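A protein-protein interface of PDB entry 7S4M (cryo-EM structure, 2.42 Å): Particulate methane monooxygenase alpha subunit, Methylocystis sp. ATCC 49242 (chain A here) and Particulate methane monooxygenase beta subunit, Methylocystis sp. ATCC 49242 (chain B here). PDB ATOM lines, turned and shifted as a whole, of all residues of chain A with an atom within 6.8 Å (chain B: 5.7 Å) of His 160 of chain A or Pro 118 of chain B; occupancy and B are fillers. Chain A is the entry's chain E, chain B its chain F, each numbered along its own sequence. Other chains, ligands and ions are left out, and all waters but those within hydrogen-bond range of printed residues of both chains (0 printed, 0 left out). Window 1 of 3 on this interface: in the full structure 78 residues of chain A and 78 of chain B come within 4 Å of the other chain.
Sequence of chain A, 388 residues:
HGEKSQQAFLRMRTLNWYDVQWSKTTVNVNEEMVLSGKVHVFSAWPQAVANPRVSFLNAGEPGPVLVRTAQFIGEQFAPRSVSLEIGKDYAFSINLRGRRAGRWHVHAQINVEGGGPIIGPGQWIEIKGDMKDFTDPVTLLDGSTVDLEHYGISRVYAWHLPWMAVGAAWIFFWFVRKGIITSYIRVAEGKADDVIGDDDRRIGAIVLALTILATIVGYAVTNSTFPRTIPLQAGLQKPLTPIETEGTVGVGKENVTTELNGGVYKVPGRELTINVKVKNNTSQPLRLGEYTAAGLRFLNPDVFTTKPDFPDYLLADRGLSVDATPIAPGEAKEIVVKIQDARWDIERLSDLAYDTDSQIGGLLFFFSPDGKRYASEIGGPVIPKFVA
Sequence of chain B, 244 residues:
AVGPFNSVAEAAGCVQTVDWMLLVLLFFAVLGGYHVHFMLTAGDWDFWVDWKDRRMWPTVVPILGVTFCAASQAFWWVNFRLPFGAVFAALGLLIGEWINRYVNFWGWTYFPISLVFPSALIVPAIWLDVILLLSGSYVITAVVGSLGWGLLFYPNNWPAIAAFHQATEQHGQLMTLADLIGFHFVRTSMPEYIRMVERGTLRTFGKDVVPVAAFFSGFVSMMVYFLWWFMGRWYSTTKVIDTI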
ATOM      1  N   ARG A 155      32.146  23.463  12.544  1.00  0.00           N
ATOM      2  CA  ARG A 155      31.887  23.946  11.193  1.00  0.00           C
ATOM      3  C   ARG A 155      30.399  23.909  10.868  1.00  0.00           C
ATOM      4  O   ARG A 155      29.866  24.837  10.246  1.00  0.00           O
ATOM      5  CB  ARG A 155      32.676  23.117  10.183  1.00  0.00           C
ATOM      6  CG  ARG A 155      32.609  23.646   8.768  1.00  0.00           C
ATOM      7  CD  ARG A 155      33.513  22.851   7.853  1.00  0.00           C
ATOM      8  NE  ARG A 155      34.889  22.847   8.332  1.00  0.00           N
ATOM      9  CZ  ARG A 155      35.791  23.765   8.020  1.00  0.00           C
ATOM     10  NH1 ARG A 155      35.496  24.779   7.224  1.00  0.00           N
ATOM     11  NH2 ARG A 155      37.019  23.664   8.519  1.00  0.00           N
ATOM     12  N   VAL A 156      29.712  22.844  11.282  1.00  0.00           N
ATOM     13  CA  VAL A 156      28.280  22.740  11.024  1.00  0.00           C
ATOM     14  C   VAL A 156      27.532  23.867  11.719  1.00  0.00           C
ATOM     15  O   VAL A 156      26.640  24.489  11.134  1.00  0.00           O
ATOM     16  CB  VAL A 156      27.757  21.360  11.455  1.00  0.00           C
ATOM     17  CG1 VAL A 156      26.244  21.354  11.484  1.00  0.00           C
ATOM     18  CG2 VAL A 156      28.274  20.288  10.519  1.00  0.00           C
ATOM     19  N   TYR A 157      27.881  24.149  12.976  1.00  0.00           N
ATOM     20  CA  TYR A 157      27.265  25.272  13.673  1.00  0.00           C
ATOM     21  C   TYR A 157      27.555  26.582  12.956  1.00  0.00           C
ATOM     22  O   TYR A 157      26.643  27.376  12.692  1.00  0.00           O
ATOM     23  CB  TYR A 157      27.768  25.337  15.113  1.00  0.00           C
ATOM     24  CG  TYR A 157      27.120  24.345  16.041  1.00  0.00           C
ATOM     25  CD1 TYR A 157      25.823  23.913  15.829  1.00  0.00           C
ATOM     26  CD2 TYR A 157      27.805  23.851  17.139  1.00  0.00           C
ATOM     27  CE1 TYR A 157      25.230  23.009  16.679  1.00  0.00           C
ATOM     28  CE2 TYR A 157      27.217  22.949  17.996  1.00  0.00           C
ATOM     29  CZ  TYR A 157      25.931  22.531  17.760  1.00  0.00           C
ATOM     30  OH  TYR A 157      25.344  21.628  18.614  1.00  0.00           O
ATOM     31  N   ALA A 158      28.824  26.817  12.616  1.00  0.00           N
ATOM     32  CA  ALA A 158      29.225  28.076  12.008  1.00  0.00           C
ATOM     33  C   ALA A 158      28.603  28.281  10.639  1.00  0.00           C
ATOM     34  O   ALA A 158      28.549  29.417  10.160  1.00  0.00           O
ATOM     35  CB  ALA A 158      30.746  28.145  11.900  1.00  0.00           C
ATOM     36  N   TRP A 159      28.158  27.213   9.987  1.00  0.00           N
ATOM     37  CA  TRP A 159      27.458  27.398   8.724  1.00  0.00           C
ATOM     38  C   TRP A 159      25.947  27.475   8.895  1.00  0.00           C
ATOM     39  O   TRP A 159      25.278  28.183   8.137  1.00  0.00           O
ATOM     40  CB  TRP A 159      27.803  26.271   7.751  1.00  0.00           C
ATOM     41  CG  TRP A 159      27.128  26.430   6.436  1.00  0.00           C
ATOM     42  CD1 TRP A 159      26.103  25.681   5.949  1.00  0.00           C
ATOM     43  CD2 TRP A 159      27.416  27.414   5.438  1.00  0.00           C
ATOM     44  NE1 TRP A 159      25.738  26.130   4.706  1.00  0.00           N
ATOM     45  CE2 TRP A 159      26.532  27.194   4.368  1.00  0.00           C
ATOM     46  CE3 TRP A 159      28.342  28.453   5.341  1.00  0.00           C
ATOM     47  CZ2 TRP A 159      26.542  27.975   3.220  1.00  0.00           C
ATOM     48  CZ3 TRP A 159      28.351  29.229   4.201  1.00  0.00           C
ATOM     49  CH2 TRP A 159      27.458  28.986   3.156  1.00  0.00           C
ATOM     50  N   HIS A 160      25.389  26.767   9.877  1.00  0.00           N
ATOM     51  CA  HIS A 160      23.938  26.692   9.992  1.00  0.00           C
ATOM     52  C   HIS A 160      23.369  27.862  10.782  1.00  0.00           C
ATOM     53  O   HIS A 160      22.431  28.523  10.328  1.00  0.00           O
ATOM     54  CB  HIS A 160      23.534  25.368  10.637  1.00  0.00           C
ATOM     55  CG  HIS A 160      23.243  24.285   9.650  1.00  0.00           C
ATOM     56  ND1 HIS A 160      21.976  23.791   9.438  1.00  0.00           N
ATOM     57  CD2 HIS A 160      24.056  23.606   8.806  1.00  0.00           C
ATOM     58  CE1 HIS A 160      22.020  22.850   8.512  1.00  0.00           C
ATOM     59  NE2 HIS A 160      23.270  22.718   8.113  1.00  0.00           N
ATOM     60  N   LEU A 161      23.913  28.124  11.969  1.00  0.00           N
ATOM     61  CA  LEU A 161      23.348  29.171  12.816  1.00  0.00           C
ATOM     62  C   LEU A 161      23.337  30.547  12.160  1.00  0.00           C
ATOM     63  O   LEU A 161      22.311  31.241  12.278  1.00  0.00           O
ATOM     64  CB  LEU A 161      24.093  29.211  14.155  1.00  0.00           C
ATOM     65  CG  LEU A 161      24.130  27.894  14.927  1.00  0.00           C
ATOM     66  CD1 LEU A 161      24.721  28.104  16.307  1.00  0.00           C
ATOM     67  CD2 LEU A 161      22.741  27.290  15.024  1.00  0.00           C
ATOM     68  N   PRO A 162      24.400  31.013  11.495  1.00  0.00           N
ATOM     69  CA  PRO A 162      24.308  32.328  10.841  1.00  0.00           C
ATOM     70  C   PRO A 162      23.198  32.418   9.813  1.00  0.00           C
ATOM     71  O   PRO A 162      22.562  33.467   9.693  1.00  0.00           O
ATOM     72  CB  PRO A 162      25.691  32.491  10.201  1.00  0.00           C
ATOM     73  CG  PRO A 162      26.576  31.681  11.051  1.00  0.00           C
ATOM     74  CD  PRO A 162      25.769  30.479  11.419  1.00  0.00           C
ATOM     75  N   TRP A 163      22.935  31.344   9.068  1.00  0.00           N
ATOM     76  CA  TRP A 163      21.867  31.402   8.077  1.00  0.00           C
ATOM     77  C   TRP A 163      20.494  31.450   8.732  1.00  0.00           C
ATOM     78  O   TRP A 163      19.601  32.151   8.243  1.00  0.00           O
ATOM     79  CB  TRP A 163      21.972  30.218   7.122  1.00  0.00           C
ATOM     80  CG  TRP A 163      22.981  30.439   6.051  1.00  0.00           C
ATOM     81  CD1 TRP A 163      24.113  29.717   5.832  1.00  0.00           C
ATOM     82  CD2 TRP A 163      22.958  31.460   5.050  1.00  0.00           C
ATOM     83  NE1 TRP A 163      24.796  30.221   4.756  1.00  0.00           N
ATOM     84  CE2 TRP A 163      24.106  31.293   4.258  1.00  0.00           C
ATOM     85  CE3 TRP A 163      22.077  32.499   4.748  1.00  0.00           C
ATOM     86  CZ2 TRP A 163      24.398  32.125   3.184  1.00  0.00           C
ATOM     87  CZ3 TRP A 163      22.365  33.322   3.682  1.00  0.00           C
ATOM     88  CH2 TRP A 163      23.515  33.132   2.912  1.00  0.00           C
ATOM     89  N   MET A 164      20.305  30.726   9.833  1.00  0.00           N
ATOM     90  CA  MET A 164      19.055  30.842  10.576  1.00  0.00           C
ATOM     91  C   MET A 164      18.880  32.252  11.117  1.00  0.00           C
ATOM     92  O   MET A 164      17.774  32.806  11.093  1.00  0.00           O
ATOM     93  CB  MET A 164      19.019  29.823  11.711  1.00  0.00           C
ATOM     94  CG  MET A 164      19.204  28.390  11.257  1.00  0.00           C
ATOM     95  SD  MET A 164      18.353  27.222  12.328  1.00  0.00           S
ATOM     96  CE  MET A 164      18.821  27.847  13.936  1.00  0.00           C
ATOM     97  N   ALA A 165      19.966  32.852  11.608  1.00  0.00           N
ATOM     98  CA  ALA A 165      19.897  34.233  12.065  1.00  0.00           C
ATOM     99  C   ALA A 165      19.538  35.171  10.921  1.00  0.00           C
ATOM    100  O   ALA A 165      18.761  36.112  11.104  1.00  0.00           O
ATOM    101  CB  ALA A 165      21.225  34.645  12.697  1.00  0.00           C
ATOM    102  N   ASP B  46      17.166  13.920   6.629  1.00  0.00           N
ATOM    103  CA  ASP B  46      17.713  14.988   7.450  1.00  0.00           C
ATOM    104  C   ASP B  46      18.276  14.452   8.756  1.00  0.00           C
ATOM    105  O   ASP B  46      19.047  15.144   9.428  1.00  0.00           O
ATOM    106  CB  ASP B  46      16.635  16.029   7.737  1.00  0.00           C
ATOM    107  CG  ASP B  46      17.090  17.431   7.424  1.00  0.00           C
ATOM    108  OD1 ASP B  46      18.269  17.594   7.057  1.00  0.00           O
ATOM    109  OD2 ASP B  46      16.277  18.369   7.546  1.00  0.00           O
ATOM    110  N   LYS B  52      22.941  11.489   3.755  1.00  0.00           N
ATOM    111  CA  LYS B  52      22.999  12.647   2.867  1.00  0.00           C
ATOM    112  C   LYS B  52      23.945  12.330   1.713  1.00  0.00           C
ATOM    113  O   LYS B  52      25.099  12.758   1.669  1.00  0.00           O
ATOM    114  CB  LYS B  52      23.441  13.882   3.639  1.00  0.00           C
ATOM    115  CG  LYS B  52      22.699  14.086   4.945  1.00  0.00           C
ATOM    116  CD  LYS B  52      22.816  15.518   5.425  1.00  0.00           C
ATOM    117  CE  LYS B  52      22.340  15.661   6.857  1.00  0.00           C
ATOM    118  NZ  LYS B  52      21.002  15.057   7.062  1.00  0.00           N
ATOM    119  N   LEU B  94      13.717  24.618  10.280  1.00  0.00           N
ATOM    120  CA  LEU B  94      15.098  24.481  10.723  1.00  0.00           C
ATOM    121  C   LEU B  94      15.227  24.732  12.217  1.00  0.00           C
ATOM    122  O   LEU B  94      15.994  24.045  12.896  1.00  0.00           O
ATOM    123  CB  LEU B  94      15.998  25.424   9.936  1.00  0.00           C
ATOM    124  CG  LEU B  94      16.572  24.774   8.681  1.00  0.00           C
ATOM    125  CD1 LEU B  94      16.999  25.825   7.683  1.00  0.00           C
ATOM    126  CD2 LEU B  94      17.732  23.868   9.041  1.00  0.00           C
ATOM    127  N   GLU B  97      13.845  21.624  13.948  1.00  0.00           N
ATOM    128  CA  GLU B  97      14.748  20.496  13.773  1.00  0.00           C
ATOM    129  C   GLU B  97      16.005  20.659  14.611  1.00  0.00           C
ATOM    130  O   GLU B  97      16.448  19.707  15.253  1.00  0.00           O
ATOM    131  CB  GLU B  97      15.107  20.336  12.299  1.00  0.00           C
ATOM    132  CG  GLU B  97      14.009  19.710  11.472  1.00  0.00           C
ATOM    133  CD  GLU B  97      14.483  19.304  10.096  1.00  0.00           C
ATOM    134  OE1 GLU B  97      14.838  20.198   9.302  1.00  0.00           O
ATOM    135  OE2 GLU B  97      14.501  18.090   9.808  1.00  0.00           O
ATOM    136  N   TRP B  98      16.595  21.854  14.622  1.00  0.00           N
ATOM    137  CA  TRP B  98      17.809  22.066  15.399  1.00  0.00           C
ATOM    138  C   TRP B  98      17.539  21.932  16.888  1.00  0.00           C
ATOM    139  O   TRP B  98      18.336  21.328  17.617  1.00  0.00           O
ATOM    140  CB  TRP B  98      18.402  23.435  15.084  1.00  0.00           C
ATOM    141  CG  TRP B  98      19.504  23.365  14.093  1.00  0.00           C
ATOM    142  CD1 TRP B  98      19.517  23.904  12.845  1.00  0.00           C
ATOM    143  CD2 TRP B  98      20.759  22.703  14.259  1.00  0.00           C
ATOM    144  NE1 TRP B  98      20.707  23.627  12.223  1.00  0.00           N
ATOM    145  CE2 TRP B  98      21.487  22.888  13.071  1.00  0.00           C
ATOM    146  CE3 TRP B  98      21.338  21.973  15.297  1.00  0.00           C
ATOM    147  CZ2 TRP B  98      22.762  22.371  12.894  1.00  0.00           C
ATOM    148  CZ3 TRP B  98      22.601  21.461  15.120  1.00  0.00           C
ATOM    149  CH2 TRP B  98      23.302  21.662  13.928  1.00  0.00           C
ATOM    150  N   ARG B 101      17.213  18.215  17.548  1.00  0.00           N
ATOM    151  CA  ARG B 101      18.502  17.539  17.455  1.00  0.00           C
ATOM    152  C   ARG B 101      19.340  17.796  18.697  1.00  0.00           C
ATOM    153  O   ARG B 101      19.953  16.872  19.243  1.00  0.00           O
ATOM    154  CB  ARG B 101      19.272  17.998  16.218  1.00  0.00           C
ATOM    155  CG  ARG B 101      18.633  17.717  14.873  1.00  0.00           C
ATOM    156  CD  ARG B 101      17.877  16.411  14.834  1.00  0.00           C
ATOM    157  NE  ARG B 101      16.827  16.436  13.822  1.00  0.00           N
ATOM    158  CZ  ARG B 101      17.042  16.368  12.516  1.00  0.00           C
ATOM    159  NH1 ARG B 101      18.262  16.268  12.017  1.00  0.00           N
ATOM    160  NH2 ARG B 101      16.003  16.398  11.687  1.00  0.00           N
ATOM    161  N   VAL B 116      23.653  13.982  13.514  1.00  0.00           N
ATOM    162  CA  VAL B 116      22.225  14.260  13.456  1.00  0.00           C
ATOM    163  C   VAL B 116      21.908  15.682  13.028  1.00  0.00           C
ATOM    164  O   VAL B 116      20.759  16.108  13.166  1.00  0.00           O
ATOM    165  CB  VAL B 116      21.546  13.950  14.803  1.00  0.00           C
ATOM    166  CG1 VAL B 116      21.635  12.470  15.102  1.00  0.00           C
ATOM    167  CG2 VAL B 116      22.192  14.756  15.908  1.00  0.00           C
ATOM    168  N   PHE B 117      22.877  16.431  12.516  1.00  0.00           N
ATOM    169  CA  PHE B 117      22.584  17.789  12.093  1.00  0.00           C
ATOM    170  C   PHE B 117      21.682  17.780  10.859  1.00  0.00           C
ATOM    171  O   PHE B 117      21.808  16.912   9.993  1.00  0.00           O
ATOM    172  CB  PHE B 117      23.871  18.555  11.804  1.00  0.00           C
ATOM    173  CG  PHE B 117      24.607  18.084  10.588  1.00  0.00           C
ATOM    174  CD1 PHE B 117      25.479  17.018  10.665  1.00  0.00           C
ATOM    175  CD2 PHE B 117      24.445  18.721   9.373  1.00  0.00           C
ATOM    176  CE1 PHE B 117      26.162  16.588   9.554  1.00  0.00           C
ATOM    177  CE2 PHE B 117      25.128  18.294   8.257  1.00  0.00           C
ATOM    178  CZ  PHE B 117      25.988  17.227   8.347  1.00  0.00           C
ATOM    179  N   PRO B 118      20.757  18.728  10.766  1.00  0.00           N
ATOM    180  CA  PRO B 118      19.842  18.768   9.624  1.00  0.00           C
ATOM    181  C   PRO B 118      20.478  19.447   8.419  1.00  0.00           C
ATOM    182  O   PRO B 118      21.606  19.937   8.463  1.00  0.00           O
ATOM    183  CB  PRO B 118      18.666  19.584  10.158  1.00  0.00           C
ATOM    184  CG  PRO B 118      19.293  20.508  11.130  1.00  0.00           C
ATOM    185  CD  PRO B 118      20.434  19.759  11.764  1.00  0.00           C
ATOM    186  N   SER B 119      19.719  19.471   7.328  1.00  0.00           N
ATOM    187  CA  SER B 119      20.169  20.091   6.092  1.00  0.00           C
ATOM    188  C   SER B 119      19.704  21.539   6.028  1.00  0.00           C
ATOM    189  O   SER B 119      18.573  21.858   6.400  1.00  0.00           O
ATOM    190  CB  SER B 119      19.647  19.323   4.880  1.00  0.00           C
ATOM    191  OG  SER B 119      18.320  18.883   5.096  1.00  0.00           O
ATOM    192  N   ALA B 120      20.587  22.408   5.549  1.00  0.00           N
ATOM    193  CA  ALA B 120      20.287  23.828   5.460  1.00  0.00           C
ATOM    194  C   ALA B 120      19.330  24.095   4.305  1.00  0.00           C
ATOM    195  O   ALA B 120      19.519  23.581   3.200  1.00  0.00           O
ATOM    196  CB  ALA B 120      21.573  24.628   5.280  1.00  0.00           C
ATOM    197  N   ASN B 157      24.519  23.394   1.207  1.00  0.00           N
ATOM    198  CA  ASN B 157      24.720  22.368   2.218  1.00  0.00           C
ATOM    199  C   ASN B 157      26.129  21.800   2.216  1.00  0.00           C
ATOM    200  O   ASN B 157      26.514  21.138   3.184  1.00  0.00           O
ATOM    201  CB  ASN B 157      23.719  21.226   2.022  1.00  0.00           C
ATOM    202  CG  ASN B 157      22.528  21.339   2.938  1.00  0.00           C
ATOM    203  OD1 ASN B 157      22.671  21.371   4.158  1.00  0.00           O
ATOM    204  ND2 ASN B 157      21.341  21.401   2.357  1.00  0.00           N
ATOM    205  N   ALA B 160      28.640  22.395   5.211  1.00  0.00           N
ATOM    206  CA  ALA B 160      28.397  21.687   6.458  1.00  0.00           C
ATOM    207  C   ALA B 160      28.668  20.193   6.379  1.00  0.00           C
ATOM    208  O   ALA B 160      28.857  19.563   7.423  1.00  0.00           O
ATOM    209  CB  ALA B 160      26.952  21.906   6.916  1.00  0.00           C
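A ring nitrogen (ND1) of His 160 of chain A sits at hydrogen-bond distance from the indole nitrogen (NE1) of Trp 98 of chain B (3.1 Å).
NE2 of His 160 of chain A sits close to O of Pro 118 of chain B, 3.3 Å away.
The side-chain carboxylate (OD2) of Asp 46 of chain B lies close to the side-chain hydroxyl (OG) of Ser 119 of chain B, at 3.2 Å.
The backbone NH of Ala 120 of chain B is in hydrogen-bond range of the side-chain amide oxygen of Asn 157 of chain B (2.7 Å).
Among the printed residues, merely in contact across the chains: Val 156 of chain A with Ala 160 of chain B, His 160 of chain A with Ala 120 of chain B, Tyr 157 of chain A with Trp 98 of chain B, Met 164 of chain A with Trp 98 of chain B, His 160 of chain A with Ser 119 of chain B, Val 156 of chain A with Phe 117 of chain B, Met 164 of chain A with Leu 94 of chain B, Val 156 of chain A with Trp 98 of chain B, His 160 of chain A with Ala 160 of chain B and Trp 159 of chain A with Ala 160 of chain B.
Of the printed residues of chain B, Trp 159 of chain A touches Ala 160 (3.99 Å).
Of the printed residues of chain B, His 160 of chain A touches Trp 98, Pro 118, Ser 119, Ala 120 and Ala 160.
Asp 46 of chain B touches none of the printed residues of chain A.
Of the printed residues of chain A, Leu 94 of chain B touches Met 164 (3.8 Å).
Arg 101 of chain B touches none of the printed residues of chain A.
Pro 118 of chain B touches just one residue of chain A: His 160 (2.9 Å).
Of the printed residues of chain A, Ala 120 of chain B touches His 160.
The nearest printed residue of chain A that does not touch Leu 94 of chain B is His 160 of chain A (4.3 Å).
Of the 13 printed residues of chain B, 7 touch a printed residue of chain A.
Printed residues of chain B that touch a printed residue of chain A: Leu 94, Trp 98, Phe 117, Pro 118, Ser 119, Ala 120 and Ala 160.
Hydrophobic or aromatic side chains of chain B within 4 Å of the printed part of chain A: Leu 94, Trp 98, Phe 117, Ala 120 and Ala 160.
Hydrophobic or aromatic side chains of chain A within 4 Å of the printed part of chain B: Val 156, Tyr 157, Trp 159, His 160 and Met 164.
Among the printed residues, 12 pairs touch across the chains.
Among the printed residues, no Asp or Glu carboxylate lies within 4 Å of a Lys or Arg side-chain nitrogen of the other chain.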
